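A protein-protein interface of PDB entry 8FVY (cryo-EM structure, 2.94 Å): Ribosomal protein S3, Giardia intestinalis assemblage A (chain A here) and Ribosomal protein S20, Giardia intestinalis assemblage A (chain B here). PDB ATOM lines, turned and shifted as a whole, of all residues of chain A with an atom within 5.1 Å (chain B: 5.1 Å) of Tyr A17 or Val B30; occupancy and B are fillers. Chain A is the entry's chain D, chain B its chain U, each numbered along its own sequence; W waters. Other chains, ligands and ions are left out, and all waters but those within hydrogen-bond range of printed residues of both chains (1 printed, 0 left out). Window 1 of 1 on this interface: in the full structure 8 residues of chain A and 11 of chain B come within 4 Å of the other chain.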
ATOM      1  N   VAL A  12      15.531  -2.929 -10.249  1.00  0.00           N
ATOM      2  CA  VAL A  12      14.626  -3.332 -11.315  1.00  0.00           C
ATOM      3  C   VAL A  12      14.015  -2.109 -11.983  1.00  0.00           C
ATOM      4  O   VAL A  12      13.895  -2.053 -13.209  1.00  0.00           O
ATOM      5  CB  VAL A  12      13.550  -4.277 -10.764  1.00  0.00           C
ATOM      6  CG1 VAL A  12      14.192  -5.350  -9.936  1.00  0.00           C
ATOM      7  CG2 VAL A  12      12.566  -3.514  -9.933  1.00  0.00           C
ATOM      8  N   TYR A  13      13.616  -1.114 -11.194  1.00  0.00           N
ATOM      9  CA  TYR A  13      13.093   0.106 -11.788  1.00  0.00           C
ATOM     10  C   TYR A  13      14.170   0.816 -12.568  1.00  0.00           C
ATOM     11  O   TYR A  13      13.920   1.373 -13.639  1.00  0.00           O
ATOM     12  CB  TYR A  13      12.544   1.041 -10.726  1.00  0.00           C
ATOM     13  CG  TYR A  13      11.541   0.428  -9.810  1.00  0.00           C
ATOM     14  CD1 TYR A  13      10.510  -0.329 -10.309  1.00  0.00           C
ATOM     15  CD2 TYR A  13      11.615   0.617  -8.448  1.00  0.00           C
ATOM     16  CE1 TYR A  13       9.589  -0.890  -9.486  1.00  0.00           C
ATOM     17  CE2 TYR A  13      10.691   0.055  -7.612  1.00  0.00           C
ATOM     18  CZ  TYR A  13       9.677  -0.699  -8.141  1.00  0.00           C
ATOM     19  OH  TYR A  13       8.739  -1.273  -7.328  1.00  0.00           O
ATOM     20  N   TYR A  14      15.377   0.823 -12.029  1.00  0.00           N
ATOM     21  CA  TYR A  14      16.444   1.550 -12.690  1.00  0.00           C
ATOM     22  C   TYR A  14      16.885   0.836 -13.956  1.00  0.00           C
ATOM     23  O   TYR A  14      17.221   1.477 -14.955  1.00  0.00           O
ATOM     24  CB  TYR A  14      17.600   1.743 -11.733  1.00  0.00           C
ATOM     25  CG  TYR A  14      17.322   2.732 -10.633  1.00  0.00           C
ATOM     26  CD1 TYR A  14      16.867   3.992 -10.916  1.00  0.00           C
ATOM     27  CD2 TYR A  14      17.531   2.407  -9.312  1.00  0.00           C
ATOM     28  CE1 TYR A  14      16.622   4.892  -9.928  1.00  0.00           C
ATOM     29  CE2 TYR A  14      17.287   3.304  -8.318  1.00  0.00           C
ATOM     30  CZ  TYR A  14      16.834   4.548  -8.634  1.00  0.00           C
ATOM     31  OH  TYR A  14      16.590   5.457  -7.639  1.00  0.00           O
ATOM     32  N   SER A  15      16.879  -0.492 -13.940  1.00  0.00           N
ATOM     33  CA  SER A  15      17.286  -1.257 -15.101  1.00  0.00           C
ATOM     34  C   SER A  15      16.161  -1.429 -16.097  1.00  0.00           C
ATOM     35  O   SER A  15      16.405  -1.866 -17.223  1.00  0.00           O
ATOM     36  CB  SER A  15      17.789  -2.616 -14.661  1.00  0.00           C
ATOM     37  OG  SER A  15      18.694  -3.145 -15.610  1.00  0.00           O
ATOM     38  N   LYS A  16      14.944  -1.112 -15.703  1.00  0.00           N
ATOM     39  CA  LYS A  16      13.810  -1.157 -16.601  1.00  0.00           C
ATOM     40  C   LYS A  16      13.603   0.156 -17.325  1.00  0.00           C
ATOM     41  O   LYS A  16      12.687   0.260 -18.142  1.00  0.00           O
ATOM     42  CB  LYS A  16      12.562  -1.530 -15.818  1.00  0.00           C
ATOM     43  CG  LYS A  16      11.475  -2.113 -16.647  1.00  0.00           C
ATOM     44  CD  LYS A  16      10.131  -1.548 -16.238  1.00  0.00           C
ATOM     45  CE  LYS A  16       9.066  -1.839 -17.273  1.00  0.00           C
ATOM     46  NZ  LYS A  16       9.516  -1.564 -18.662  1.00  0.00           N
ATOM     47  N   TYR A  17      14.416   1.158 -17.021  1.00  0.00           N
ATOM     48  CA  TYR A  17      14.450   2.426 -17.727  1.00  0.00           C
ATOM     49  C   TYR A  17      15.588   2.454 -18.722  1.00  0.00           C
ATOM     50  O   TYR A  17      15.431   2.940 -19.844  1.00  0.00           O
ATOM     51  CB  TYR A  17      14.625   3.565 -16.731  1.00  0.00           C
ATOM     52  CG  TYR A  17      14.263   4.919 -17.240  1.00  0.00           C
ATOM     53  CD1 TYR A  17      12.960   5.351 -17.241  1.00  0.00           C
ATOM     54  CD2 TYR A  17      15.228   5.779 -17.691  1.00  0.00           C
ATOM     55  CE1 TYR A  17      12.633   6.589 -17.699  1.00  0.00           C
ATOM     56  CE2 TYR A  17      14.909   7.011 -18.147  1.00  0.00           C
ATOM     57  CZ  TYR A  17      13.611   7.414 -18.150  1.00  0.00           C
ATOM     58  OH  TYR A  17      13.285   8.656 -18.610  1.00  0.00           O
ATOM     59  N   LEU A  18      16.730   1.920 -18.310  1.00  0.00           N
ATOM     60  CA  LEU A  18      17.906   1.888 -19.157  1.00  0.00           C
ATOM     61  C   LEU A  18      17.670   1.080 -20.416  1.00  0.00           C
ATOM     62  O   LEU A  18      18.029   1.505 -21.517  1.00  0.00           O
ATOM     63  CB  LEU A  18      19.052   1.286 -18.373  1.00  0.00           C
ATOM     64  CG  LEU A  18      20.445   1.484 -18.930  1.00  0.00           C
ATOM     65  CD1 LEU A  18      20.836   2.921 -18.879  1.00  0.00           C
ATOM     66  CD2 LEU A  18      21.409   0.636 -18.171  1.00  0.00           C
ATOM     67  N   ASN A  19      17.078  -0.097 -20.270  1.00  0.00           N
ATOM     68  CA  ASN A  19      16.843  -0.963 -21.412  1.00  0.00           C
ATOM     69  C   ASN A  19      16.003  -0.265 -22.457  1.00  0.00           C
ATOM     70  O   ASN A  19      16.252  -0.386 -23.661  1.00  0.00           O
ATOM     71  CB  ASN A  19      16.150  -2.227 -20.948  1.00  0.00           C
ATOM     72  CG  ASN A  19      16.941  -2.969 -19.919  1.00  0.00           C
ATOM     73  OD1 ASN A  19      17.971  -2.496 -19.448  1.00  0.00           O
ATOM     74  ND2 ASN A  19      16.468  -4.144 -19.560  1.00  0.00           N
ATOM     75  N   ASP A  20      14.992   0.456 -22.011  1.00  0.00           N
ATOM     76  CA  ASP A  20      14.073   1.116 -22.911  1.00  0.00           C
ATOM     77  C   ASP A  20      14.674   2.351 -23.554  1.00  0.00           C
ATOM     78  O   ASP A  20      14.282   2.718 -24.665  1.00  0.00           O
ATOM     79  CB  ASP A  20      12.813   1.436 -22.137  1.00  0.00           C
ATOM     80  CG  ASP A  20      12.095   0.192 -21.701  1.00  0.00           C
ATOM     81  OD1 ASP A  20      12.780  -0.744 -21.244  1.00  0.00           O
ATOM     82  OD2 ASP A  20      10.858   0.134 -21.825  1.00  0.00           O
ATOM     83  N   CYS A  21      15.609   3.003 -22.877  1.00  0.00           N
ATOM     84  CA  CYS A  21      16.346   4.082 -23.512  1.00  0.00           C
ATOM     85  C   CYS A  21      17.202   3.557 -24.648  1.00  0.00           C
ATOM     86  O   CYS A  21      17.327   4.201 -25.694  1.00  0.00           O
ATOM     87  CB  CYS A  21      17.198   4.797 -22.481  1.00  0.00           C
ATOM     88  SG  CYS A  21      16.290   5.874 -21.376  1.00  0.00           S
ATOM     89  N   ILE B  28       5.276   4.854  -8.080  1.00  0.00           N
ATOM     90  CA  ILE B  28       6.686   5.114  -8.332  1.00  0.00           C
ATOM     91  C   ILE B  28       6.846   5.657  -9.737  1.00  0.00           C
ATOM     92  O   ILE B  28       6.316   5.082 -10.692  1.00  0.00           O
ATOM     93  CB  ILE B  28       7.538   3.860  -8.142  1.00  0.00           C
ATOM     94  CG1 ILE B  28       7.428   3.367  -6.719  1.00  0.00           C
ATOM     95  CG2 ILE B  28       8.934   4.139  -8.473  1.00  0.00           C
ATOM     96  CD1 ILE B  28       6.967   1.994  -6.597  1.00  0.00           C
ATOM     97  N   VAL B  29       7.588   6.751  -9.862  1.00  0.00           N
ATOM     98  CA  VAL B  29       7.858   7.402 -11.134  1.00  0.00           C
ATOM     99  C   VAL B  29       9.344   7.701 -11.232  1.00  0.00           C
ATOM    100  O   VAL B  29       9.961   8.139 -10.258  1.00  0.00           O
ATOM    101  CB  VAL B  29       7.029   8.680 -11.298  1.00  0.00           C
ATOM    102  CG1 VAL B  29       6.538   9.128  -9.985  1.00  0.00           C
ATOM    103  CG2 VAL B  29       7.837   9.755 -11.943  1.00  0.00           C
ATOM    104  N   VAL B  30       9.899   7.501 -12.421  1.00  0.00           N
ATOM    105  CA  VAL B  30      11.328   7.573 -12.675  1.00  0.00           C
ATOM    106  C   VAL B  30      11.576   8.413 -13.912  1.00  0.00           C
ATOM    107  O   VAL B  30      10.830   8.321 -14.890  1.00  0.00           O
ATOM    108  CB  VAL B  30      11.942   6.182 -12.873  1.00  0.00           C
ATOM    109  CG1 VAL B  30      13.382   6.300 -13.131  1.00  0.00           C
ATOM    110  CG2 VAL B  30      11.696   5.340 -11.704  1.00  0.00           C
ATOM    111  N   GLY B  31      12.640   9.199 -13.883  1.00  0.00           N
ATOM    112  CA  GLY B  31      12.998  10.011 -15.023  1.00  0.00           C
ATOM    113  C   GLY B  31      14.452  10.405 -14.988  1.00  0.00           C
ATOM    114  O   GLY B  31      15.093  10.424 -13.936  1.00  0.00           O
ATOM    115  N   LYS B  32      14.960  10.746 -16.166  1.00  0.00           N
ATOM    116  CA  LYS B  32      16.346  11.135 -16.327  1.00  0.00           C
ATOM    117  C   LYS B  32      16.544  12.637 -16.322  1.00  0.00           C
ATOM    118  O   LYS B  32      17.669  13.092 -16.105  1.00  0.00           O
ATOM    119  CB  LYS B  32      16.918  10.560 -17.624  1.00  0.00           C
ATOM    120  CG  LYS B  32      16.309  11.097 -18.877  1.00  0.00           C
ATOM    121  CD  LYS B  32      17.137  10.784 -20.082  1.00  0.00           C
ATOM    122  CE  LYS B  32      16.634   9.570 -20.829  1.00  0.00           C
ATOM    123  NZ  LYS B  32      17.490   9.198 -21.984  1.00  0.00           N
ATOM    124  N   VAL B  37       9.943  15.584 -14.180  1.00  0.00           N
ATOM    125  CA  VAL B  37       9.707  14.823 -12.968  1.00  0.00           C
ATOM    126  C   VAL B  37       9.070  15.718 -11.929  1.00  0.00           C
ATOM    127  O   VAL B  37       8.174  15.295 -11.191  1.00  0.00           O
ATOM    128  CB  VAL B  37      11.024  14.207 -12.474  1.00  0.00           C
ATOM    129  CG1 VAL B  37      10.772  13.324 -11.350  1.00  0.00           C
ATOM    130  CG2 VAL B  37      11.668  13.415 -13.552  1.00  0.00           C
ATOM    131  N   MET B  87      19.487   9.714 -12.631  1.00  0.00           N
ATOM    132  CA  MET B  87      18.129   9.193 -12.630  1.00  0.00           C
ATOM    133  C   MET B  87      17.431   9.614 -11.354  1.00  0.00           C
ATOM    134  O   MET B  87      17.892   9.299 -10.254  1.00  0.00           O
ATOM    135  CB  MET B  87      18.119   7.679 -12.765  1.00  0.00           C
ATOM    136  CG  MET B  87      18.111   7.211 -14.172  1.00  0.00           C
ATOM    137  SD  MET B  87      17.319   5.631 -14.392  1.00  0.00           S
ATOM    138  CE  MET B  87      18.712   4.774 -15.087  1.00  0.00           C
ATOM    139  N   TYR B  88      16.318  10.308 -11.506  1.00  0.00           N
ATOM    140  CA  TYR B  88      15.571  10.852 -10.396  1.00  0.00           C
ATOM    141  C   TYR B  88      14.336  10.001 -10.166  1.00  0.00           C
ATOM    142  O   TYR B  88      13.710   9.532 -11.117  1.00  0.00           O
ATOM    143  CB  TYR B  88      15.180  12.292 -10.684  1.00  0.00           C
ATOM    144  CG  TYR B  88      16.315  13.165 -11.099  1.00  0.00           C
ATOM    145  CD1 TYR B  88      16.748  13.181 -12.401  1.00  0.00           C
ATOM    146  CD2 TYR B  88      16.955  13.970 -10.194  1.00  0.00           C
ATOM    147  CE1 TYR B  88      17.782  13.969 -12.790  1.00  0.00           C
ATOM    148  CE2 TYR B  88      17.987  14.757 -10.568  1.00  0.00           C
ATOM    149  CZ  TYR B  88      18.402  14.758 -11.867  1.00  0.00           C
ATOM    150  OH  TYR B  88      19.445  15.563 -12.240  1.00  0.00           O
ATOM    151  N   LYS B  89      13.991   9.800  -8.902  1.00  0.00           N
ATOM    152  CA  LYS B  89      12.928   8.886  -8.533  1.00  0.00           C
ATOM    153  C   LYS B  89      12.116   9.490  -7.410  1.00  0.00           C
ATOM    154  O   LYS B  89      12.673   9.966  -6.420  1.00  0.00           O
ATOM    155  CB  LYS B  89      13.489   7.537  -8.106  1.00  0.00           C
ATOM    156  CG  LYS B  89      12.468   6.460  -8.003  1.00  0.00           C
ATOM    157  CD  LYS B  89      13.000   5.245  -7.329  1.00  0.00           C
ATOM    158  CE  LYS B  89      12.781   5.307  -5.865  1.00  0.00           C
ATOM    159  NZ  LYS B  89      13.181   4.065  -5.201  1.00  0.00           N
ATOM    160  N   VAL B 116       7.971  10.706 -21.653  1.00  0.00           N
ATOM    161  CA  VAL B 116       8.915   9.813 -20.985  1.00  0.00           C
ATOM    162  C   VAL B 116       8.882  10.084 -19.491  1.00  0.00           C
ATOM    163  O   VAL B 116       9.361  11.125 -19.029  1.00  0.00           O
ATOM    164  CB  VAL B 116      10.328   9.966 -21.517  1.00  0.00           C
ATOM    165  CG1 VAL B 116      11.279   9.345 -20.538  1.00  0.00           C
ATOM    166  CG2 VAL B 116      10.408   9.311 -22.845  1.00  0.00           C
ATOM    167  N   THR B 117       8.338   9.144 -18.726  1.00  0.00           N
ATOM    168  CA  THR B 117       8.452   9.204 -17.282  1.00  0.00           C
ATOM    169  C   THR B 117       7.834   7.916 -16.745  1.00  0.00           C
ATOM    170  O   THR B 117       6.637   7.877 -16.459  1.00  0.00           O
ATOM    171  CB  THR B 117       7.774  10.440 -16.733  1.00  0.00           C
ATOM    172  OG1 THR B 117       8.270  11.601 -17.403  1.00  0.00           O
ATOM    173  CG2 THR B 117       8.078  10.587 -15.297  1.00  0.00           C
ATOM    174  N   VAL B 118       8.663   6.885 -16.604  1.00  0.00           N
ATOM    175  CA  VAL B 118       8.176   5.560 -16.250  1.00  0.00           C
ATOM    176  C   VAL B 118       7.362   5.614 -14.972  1.00  0.00           C
ATOM    177  O   VAL B 118       7.681   6.361 -14.044  1.00  0.00           O
ATOM    178  CB  VAL B 118       9.374   4.603 -16.134  1.00  0.00           C
ATOM    179  CG1 VAL B 118       9.086   3.459 -15.212  1.00  0.00           C
ATOM    180  CG2 VAL B 118       9.752   4.076 -17.492  1.00  0.00           C
HETATM  181  O   HOH W   1      12.635  11.909 -18.819  1.00  0.00           O
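Water W1 lies within hydrogen-bond range of OH of Tyr A17 and O of Val B116.
The side-chain sulfur of Cys A21 sits at hydrogen-bond distance from the side-chain amino group of Lys B32, at 3.6 Å.
Ile B28 touches Tyr A13 (CD1 to OH, 3.8 Å).
CE of Met B87 touches O of Tyr A14, 3.6 Å away.
Tyr A14 touches Lys B89.
CE1 of Tyr A17 touches O of Val B30, 3.8 Å away.
Gly B31 touches Tyr A17 (CA to OH, 3.8 Å).
Tyr A17 touches Lys B32 (OH to N, 3.6 Å).
CD2 of Tyr A17 touches SD of Met B87, 3.9 Å away.
OH of Tyr A17 touches CG1 of Val B116 (2.9 Å).
CD1 of Tyr A17 touches CG2 of Val B118, at 3.5 Å.
O of Tyr A17 sits at hydrogen-bond distance from SG of Cys A21, 3.4 Å away.
N of Tyr B88 sits at hydrogen-bond distance from O of Gly B31 (2.7 Å).
The backbone NH of Val B30 is in hydrogen-bond range of the backbone carbonyl oxygen of Val B118 (3.0 Å).
Of the 12 printed residues of chain B, 8 touch a printed residue of chain A.
Printed residues of chain B that touch a printed residue of chain A: Ile B28, Val B30, Gly B31, Lys B32, Met B87, Lys B89, Val B116 and Val B118.
Printed residues of chain A that touch a printed residue of chain B: Tyr A13, Tyr A14, Tyr A17 and Cys A21.
Hydrophobic or aromatic side chains of chain A that line the printed part of chain B: Tyr A13, Tyr A14 and Tyr A17.
Among the printed residues, 10 pairs touch across the chains.
Tyr A17 touches just these residues of chain B: Val B30 (3.8 Å), Gly B31 (3.8 Å), Lys B32 (3.6 Å), Met B87 (3.9 Å), Val B116 (2.9 Å) and Val B118 (3.5 Å).
Of chain A, only Tyr A17 (3.8 Å) comes within 4 Å of Val B30.
Of the printed residues of chain A, Lys B32 touches Tyr A17 (3.6 Å) and Cys A21 (3.6 Å).
Printed residues of chain A within 4 Å of Val B118: Tyr A17 (3.5 Å).
The nearest residue of chain A that does not touch Val B30 is Tyr A13 (4.5 Å).
The nearest printed residue of chain A that does not touch Lys B89 is Tyr A13 (5.0 Å).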
